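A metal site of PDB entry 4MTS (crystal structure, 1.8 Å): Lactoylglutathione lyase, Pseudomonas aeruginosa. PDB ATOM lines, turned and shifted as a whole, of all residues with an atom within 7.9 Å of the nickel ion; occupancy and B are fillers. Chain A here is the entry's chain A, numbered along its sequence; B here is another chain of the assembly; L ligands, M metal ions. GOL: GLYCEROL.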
ATOM      1  N   GLY A  73      31.143  15.878 -28.437  1.00  0.00           N
ATOM      2  CA  GLY A  73      29.954  16.600 -27.986  1.00  0.00           C
ATOM      3  C   GLY A  73      28.775  16.562 -28.911  1.00  0.00           C
ATOM      4  O   GLY A  73      27.933  15.668 -28.829  1.00  0.00           O
ATOM      5  N   HIS A  74      28.774  17.485 -29.866  1.00  0.00           N
ATOM      6  CA  HIS A  74      27.668  17.618 -30.788  1.00  0.00           C
ATOM      7  C   HIS A  74      28.014  18.514 -31.922  1.00  0.00           C
ATOM      8  O   HIS A  74      29.102  19.103 -31.942  1.00  0.00           O
ATOM      9  CB  HIS A  74      26.481  18.255 -30.037  1.00  0.00           C
ATOM     10  CG  HIS A  74      26.836  19.527 -29.308  1.00  0.00           C
ATOM     11  ND1 HIS A  74      27.032  19.531 -27.945  1.00  0.00           N
ATOM     12  CD2 HIS A  74      26.970  20.796 -29.777  1.00  0.00           C
ATOM     13  CE1 HIS A  74      27.308  20.790 -27.621  1.00  0.00           C
ATOM     14  NE2 HIS A  74      27.280  21.586 -28.684  1.00  0.00           N
ATOM     15  N   LEU A  75      27.099  18.585 -32.891  1.00  0.00           N
ATOM     16  CA  LEU A  75      27.175  19.506 -33.990  1.00  0.00           C
ATOM     17  C   LEU A  75      26.001  20.490 -33.721  1.00  0.00           C
ATOM     18  O   LEU A  75      24.864  20.060 -33.501  1.00  0.00           O
ATOM     19  CB  LEU A  75      26.964  18.784 -35.352  1.00  0.00           C
ATOM     20  CG  LEU A  75      27.078  19.771 -36.562  1.00  0.00           C
ATOM     21  CD1 LEU A  75      28.540  20.157 -36.810  1.00  0.00           C
ATOM     22  CD2 LEU A  75      26.542  19.112 -37.850  1.00  0.00           C
ATOM     23  N   ALA A  76      26.262  21.775 -33.729  1.00  0.00           N
ATOM     24  CA  ALA A  76      25.208  22.749 -33.460  1.00  0.00           C
ATOM     25  C   ALA A  76      24.768  23.414 -34.768  1.00  0.00           C
ATOM     26  O   ALA A  76      25.598  23.770 -35.604  1.00  0.00           O
ATOM     27  CB  ALA A  76      25.695  23.804 -32.490  1.00  0.00           C
ATOM     28  N   ILE A  77      23.457  23.594 -34.923  1.00  0.00           N
ATOM     29  CA  ILE A  77      22.856  24.213 -36.129  1.00  0.00           C
ATOM     30  C   ILE A  77      21.949  25.385 -35.733  1.00  0.00           C
ATOM     31  O   ILE A  77      21.215  25.306 -34.763  1.00  0.00           O
ATOM     32  CB  ILE A  77      22.098  23.142 -36.958  1.00  0.00           C
ATOM     33  CG1 ILE A  77      23.101  22.036 -37.435  1.00  0.00           C
ATOM     34  CG2 ILE A  77      21.413  23.765 -38.180  1.00  0.00           C
ATOM     35  CD1 ILE A  77      22.408  20.757 -37.859  1.00  0.00           C
ATOM     36  N   ILE A 110      17.122  26.563 -27.119  1.00  0.00           N
ATOM     37  CA  ILE A 110      17.904  25.413 -27.577  1.00  0.00           C
ATOM     38  C   ILE A 110      17.051  24.146 -27.555  1.00  0.00           C
ATOM     39  O   ILE A 110      16.107  24.022 -26.758  1.00  0.00           O
ATOM     40  CB  ILE A 110      19.199  25.269 -26.675  1.00  0.00           C
ATOM     41  CG1 ILE A 110      20.121  26.516 -26.829  1.00  0.00           C
ATOM     42  CG2 ILE A 110      19.993  23.983 -26.986  1.00  0.00           C
ATOM     43  CD1 ILE A 110      21.270  26.588 -25.909  1.00  0.00           C
ATOM     44  N   PHE A 112      17.697  19.628 -28.568  1.00  0.00           N
ATOM     45  CA  PHE A 112      18.635  18.592 -28.944  1.00  0.00           C
ATOM     46  C   PHE A 112      17.944  17.478 -29.663  1.00  0.00           C
ATOM     47  O   PHE A 112      16.897  16.989 -29.225  1.00  0.00           O
ATOM     48  CB  PHE A 112      19.376  18.021 -27.742  1.00  0.00           C
ATOM     49  CG  PHE A 112      20.632  18.791 -27.415  1.00  0.00           C
ATOM     50  CD1 PHE A 112      21.853  18.410 -27.962  1.00  0.00           C
ATOM     51  CD2 PHE A 112      20.595  19.873 -26.549  1.00  0.00           C
ATOM     52  CE1 PHE A 112      23.028  19.082 -27.607  1.00  0.00           C
ATOM     53  CE2 PHE A 112      21.774  20.565 -26.216  1.00  0.00           C
ATOM     54  CZ  PHE A 112      22.971  20.168 -26.764  1.00  0.00           C
ATOM     55  N   GLU A 122      22.668  19.882 -31.708  1.00  0.00           N
ATOM     56  CA  GLU A 122      22.177  21.000 -30.899  1.00  0.00           C
ATOM     57  C   GLU A 122      21.537  22.019 -31.823  1.00  0.00           C
ATOM     58  O   GLU A 122      22.167  22.511 -32.778  1.00  0.00           O
ATOM     59  CB  GLU A 122      23.370  21.625 -30.149  1.00  0.00           C
ATOM     60  CG  GLU A 122      23.012  22.801 -29.241  1.00  0.00           C
ATOM     61  CD  GLU A 122      24.204  23.243 -28.408  1.00  0.00           C
ATOM     62  OE1 GLU A 122      25.226  23.635 -29.008  1.00  0.00           O
ATOM     63  OE2 GLU A 122      24.160  23.086 -27.170  1.00  0.00           O
ATOM     64  N   LEU A 123      20.280  22.348 -31.550  1.00  0.00           N
ATOM     65  CA  LEU A 123      19.579  23.385 -32.324  1.00  0.00           C
ATOM     66  C   LEU A 123      19.575  24.676 -31.510  1.00  0.00           C
ATOM     67  O   LEU A 123      19.185  24.658 -30.347  1.00  0.00           O
ATOM     68  CB  LEU A 123      18.140  22.960 -32.639  1.00  0.00           C
ATOM     69  CG  LEU A 123      17.945  21.599 -33.282  1.00  0.00           C
ATOM     70  CD1 LEU A 123      16.437  21.347 -33.540  1.00  0.00           C
ATOM     71  CD2 LEU A 123      18.762  21.455 -34.572  1.00  0.00           C
ATOM     72  N   ILE A 124      20.021  25.773 -32.111  1.00  0.00           N
ATOM     73  CA  ILE A 124      20.059  27.068 -31.425  1.00  0.00           C
ATOM     74  C   ILE A 124      19.250  28.053 -32.221  1.00  0.00           C
ATOM     75  O   ILE A 124      19.546  28.319 -33.386  1.00  0.00           O
ATOM     76  CB  ILE A 124      21.507  27.563 -31.164  1.00  0.00           C
ATOM     77  CG1 ILE A 124      22.321  26.487 -30.421  1.00  0.00           C
ATOM     78  CG2 ILE A 124      21.474  28.920 -30.363  1.00  0.00           C
ATOM     79  CD1 ILE A 124      23.840  26.849 -30.104  1.00  0.00           C
ATOM     80  N   GLN A 129      21.186  33.076 -29.508  1.00  0.00           N
ATOM     81  CA  GLN A 129      22.551  32.622 -29.213  1.00  0.00           C
ATOM     82  C   GLN A 129      23.389  33.630 -28.404  1.00  0.00           C
ATOM     83  O   GLN A 129      24.057  33.245 -27.450  1.00  0.00           O
ATOM     84  CB  GLN A 129      23.293  32.217 -30.503  1.00  0.00           C
ATOM     85  CG  GLN A 129      24.678  31.638 -30.217  1.00  0.00           C
ATOM     86  CD  GLN A 129      25.263  30.943 -31.406  1.00  0.00           C
ATOM     87  OE1 GLN A 129      25.642  31.549 -32.414  1.00  0.00           O
ATOM     88  NE2 GLN A 129      25.371  29.636 -31.290  1.00  0.00           N
ATOM     89  N   LEU B   4      26.757  25.991 -36.770  1.00  0.00           N
ATOM     90  CA  LEU B   4      27.342  26.949 -35.841  1.00  0.00           C
ATOM     91  C   LEU B   4      28.664  26.519 -35.261  1.00  0.00           C
ATOM     92  O   LEU B   4      29.560  27.351 -35.108  1.00  0.00           O
ATOM     93  CB  LEU B   4      26.371  27.252 -34.699  1.00  0.00           C
ATOM     94  CG  LEU B   4      25.113  28.033 -35.069  1.00  0.00           C
ATOM     95  CD1 LEU B   4      24.110  27.947 -33.957  1.00  0.00           C
ATOM     96  CD2 LEU B   4      25.471  29.468 -35.427  1.00  0.00           C
ATOM     97  N   HIS B   5      28.753  25.253 -34.815  1.00  0.00           N
ATOM     98  CA  HIS B   5      29.979  24.728 -34.243  1.00  0.00           C
ATOM     99  C   HIS B   5      29.955  23.209 -34.097  1.00  0.00           C
ATOM    100  O   HIS B   5      28.918  22.583 -34.169  1.00  0.00           O
ATOM    101  CB  HIS B   5      30.231  25.351 -32.831  1.00  0.00           C
ATOM    102  CG  HIS B   5      29.136  25.179 -31.816  1.00  0.00           C
ATOM    103  ND1 HIS B   5      28.272  26.213 -31.517  1.00  0.00           N
ATOM    104  CD2 HIS B   5      28.891  24.147 -30.969  1.00  0.00           C
ATOM    105  CE1 HIS B   5      27.491  25.766 -30.545  1.00  0.00           C
ATOM    106  NE2 HIS B   5      27.842  24.538 -30.148  1.00  0.00           N
ATOM    107  N   SER B   6      31.138  22.655 -33.872  1.00  0.00           N
ATOM    108  CA  SER B   6      31.331  21.270 -33.472  1.00  0.00           C
ATOM    109  C   SER B   6      31.851  21.412 -32.011  1.00  0.00           C
ATOM    110  O   SER B   6      32.633  22.343 -31.755  1.00  0.00           O
ATOM    111  CB  SER B   6      32.383  20.586 -34.330  1.00  0.00           C
ATOM    112  OG  SER B   6      32.561  19.273 -33.818  1.00  0.00           O
ATOM    113  N   MET B   7      31.367  20.592 -31.083  1.00  0.00           N
ATOM    114  CA  MET B   7      31.796  20.648 -29.666  1.00  0.00           C
ATOM    115  C   MET B   7      32.593  19.386 -29.306  1.00  0.00           C
ATOM    116  O   MET B   7      32.176  18.283 -29.652  1.00  0.00           O
ATOM    117  CB  MET B   7      30.581  20.750 -28.717  1.00  0.00           C
ATOM    118  CG  MET B   7      30.985  21.074 -27.233  1.00  0.00           C
ATOM    119  SD  MET B   7      31.458  19.606 -26.295  1.00  0.00           S
ATOM    120  CE  MET B   7      29.901  19.181 -25.611  1.00  0.00           C
ATOM    121  N   LEU B   8      33.754  19.560 -28.635  1.00  0.00           N
ATOM    122  CA  LEU B   8      34.594  18.491 -28.080  1.00  0.00           C
ATOM    123  C   LEU B   8      34.801  18.777 -26.599  1.00  0.00           C
ATOM    124  O   LEU B   8      35.037  19.940 -26.210  1.00  0.00           O
ATOM    125  CB  LEU B   8      35.983  18.459 -28.749  1.00  0.00           C
ATOM    126  CG  LEU B   8      35.946  18.277 -30.286  1.00  0.00           C
ATOM    127  CD1 LEU B   8      37.388  18.366 -30.859  1.00  0.00           C
ATOM    128  CD2 LEU B   8      35.295  16.909 -30.660  1.00  0.00           C
ATOM    129  N   ARG B  30      35.468  33.499 -27.639  1.00  0.00           N
ATOM    130  CA  ARG B  30      34.528  33.635 -26.515  1.00  0.00           C
ATOM    131  C   ARG B  30      34.891  32.520 -25.530  1.00  0.00           C
ATOM    132  O   ARG B  30      35.345  31.434 -25.924  1.00  0.00           O
ATOM    133  CB  ARG B  30      33.109  33.432 -27.105  1.00  0.00           C
ATOM    134  CG  ARG B  30      31.922  33.510 -26.160  1.00  0.00           C
ATOM    135  CD  ARG B  30      30.659  33.880 -26.903  1.00  0.00           C
ATOM    136  NE  ARG B  30      30.283  32.899 -27.950  1.00  0.00           N
ATOM    137  CZ  ARG B  30      29.327  31.992 -27.796  1.00  0.00           C
ATOM    138  NH1 ARG B  30      28.637  31.914 -26.659  1.00  0.00           N
ATOM    139  NH2 ARG B  30      29.022  31.171 -28.795  1.00  0.00           N
ATOM    140  N   LEU B  41      32.945  26.892 -21.156  1.00  0.00           N
ATOM    141  CA  LEU B  41      32.935  26.786 -22.611  1.00  0.00           C
ATOM    142  C   LEU B  41      33.975  27.723 -23.196  1.00  0.00           C
ATOM    143  O   LEU B  41      34.168  28.821 -22.683  1.00  0.00           O
ATOM    144  CB  LEU B  41      31.591  27.108 -23.224  1.00  0.00           C
ATOM    145  CG  LEU B  41      30.397  26.249 -22.806  1.00  0.00           C
ATOM    146  CD1 LEU B  41      29.121  26.672 -23.572  1.00  0.00           C
ATOM    147  CD2 LEU B  41      30.717  24.757 -22.987  1.00  0.00           C
ATOM    148  N   PHE B  43      35.309  29.000 -27.290  1.00  0.00           N
ATOM    149  CA  PHE B  43      35.052  28.966 -28.727  1.00  0.00           C
ATOM    150  C   PHE B  43      36.261  29.501 -29.432  1.00  0.00           C
ATOM    151  O   PHE B  43      36.676  30.646 -29.203  1.00  0.00           O
ATOM    152  CB  PHE B  43      33.829  29.793 -29.087  1.00  0.00           C
ATOM    153  CG  PHE B  43      32.564  29.278 -28.487  1.00  0.00           C
ATOM    154  CD1 PHE B  43      32.196  29.641 -27.193  1.00  0.00           C
ATOM    155  CD2 PHE B  43      31.703  28.476 -29.225  1.00  0.00           C
ATOM    156  CE1 PHE B  43      30.988  29.209 -26.644  1.00  0.00           C
ATOM    157  CE2 PHE B  43      30.501  28.033 -28.658  1.00  0.00           C
ATOM    158  CZ  PHE B  43      30.147  28.414 -27.390  1.00  0.00           C
ATOM    159  N   GLU B  56      33.757  24.515 -30.447  1.00  0.00           N
ATOM    160  CA  GLU B  56      33.377  24.717 -29.051  1.00  0.00           C
ATOM    161  C   GLU B  56      34.116  23.683 -28.195  1.00  0.00           C
ATOM    162  O   GLU B  56      34.076  22.486 -28.487  1.00  0.00           O
ATOM    163  CB  GLU B  56      31.857  24.534 -28.902  1.00  0.00           C
ATOM    164  CG  GLU B  56      31.372  24.743 -27.470  1.00  0.00           C
ATOM    165  CD  GLU B  56      29.864  24.709 -27.324  1.00  0.00           C
ATOM    166  OE1 GLU B  56      29.236  23.734 -27.785  1.00  0.00           O
ATOM    167  OE2 GLU B  56      29.308  25.679 -26.773  1.00  0.00           O
ATOM    168  N   LEU B  57      34.789  24.138 -27.139  1.00  0.00           N
ATOM    169  CA  LEU B  57      35.496  23.220 -26.226  1.00  0.00           C
ATOM    170  C   LEU B  57      34.811  23.250 -24.850  1.00  0.00           C
ATOM    171  O   LEU B  57      34.584  24.337 -24.327  1.00  0.00           O
ATOM    172  CB  LEU B  57      36.954  23.664 -26.094  1.00  0.00           C
ATOM    173  CG  LEU B  57      37.764  23.694 -27.411  1.00  0.00           C
ATOM    174  CD1 LEU B  57      39.205  24.201 -27.145  1.00  0.00           C
ATOM    175  CD2 LEU B  57      37.812  22.323 -28.032  1.00  0.00           C
ATOM    176  N   THR B  58      34.460  22.086 -24.308  1.00  0.00           N
ATOM    177  CA  THR B  58      33.786  22.054 -23.009  1.00  0.00           C
ATOM    178  C   THR B  58      34.764  21.476 -22.012  1.00  0.00           C
ATOM    179  O   THR B  58      35.283  20.366 -22.185  1.00  0.00           O
ATOM    180  CB  THR B  58      32.472  21.220 -23.051  1.00  0.00           C
ATOM    181  OG1 THR B  58      31.606  21.740 -24.048  1.00  0.00           O
ATOM    182  CG2 THR B  58      31.721  21.251 -21.723  1.00  0.00           C
HETATM  183  C1  GOL L   1      25.847  24.610 -24.247  1.00  0.00           C
HETATM  184  O1  GOL L   1      24.498  24.198 -24.370  1.00  0.00           O
HETATM  185  C2  GOL L   1      26.550  24.648 -25.581  1.00  0.00           C
HETATM  186  O2  GOL L   1      26.563  23.364 -26.212  1.00  0.00           O
HETATM  187  C3  GOL L   1      26.022  25.668 -26.555  1.00  0.00           C
HETATM  188  O3  GOL L   1      26.957  25.766 -27.625  1.00  0.00           O
HETATM  189 NI    NI M   1      27.253  23.727 -28.414  1.00  0.00          NI
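Of the 22 residues printed, 4 come within 4 Å of the nickel ion.
The backbone carbonyl oxygen of Glu 56 of chain B sits at hydrogen-bond distance from the backbone NH of Leu 8 of chain B (2.9 Å). The backbone carbonyl oxygen (O) of His 5 of chain B lies within hydrogen-bond range of the backbone NH (N) of Ala 76 (2.8 Å). The backbone carbonyl oxygen of His 74 sits at hydrogen-bond distance from the backbone NH of Met 7 of chain B. N of Glu 122 lies within hydrogen-bond range of O of Leu 75 (2.8 Å). The backbone NH of Glu 56 of chain B lies within hydrogen-bond range of the backbone carbonyl oxygen of Ser 6 of chain B, 2.8 Å away. The backbone carbonyl oxygen of Glu 122 lies within hydrogen-bond range of the backbone NH of Ile 77 (2.7 Å).
The nickel ion is bound by NE2 of His 5 of chain B (2.0 Å), OE1 of Glu 56 of chain B (2.1 Å), OE1 of Glu 122 (2.1 Å), NE2 of His 74 (2.2 Å), O3 of the ligand (2.2 Å) and O2 of the ligand (2.3 Å).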
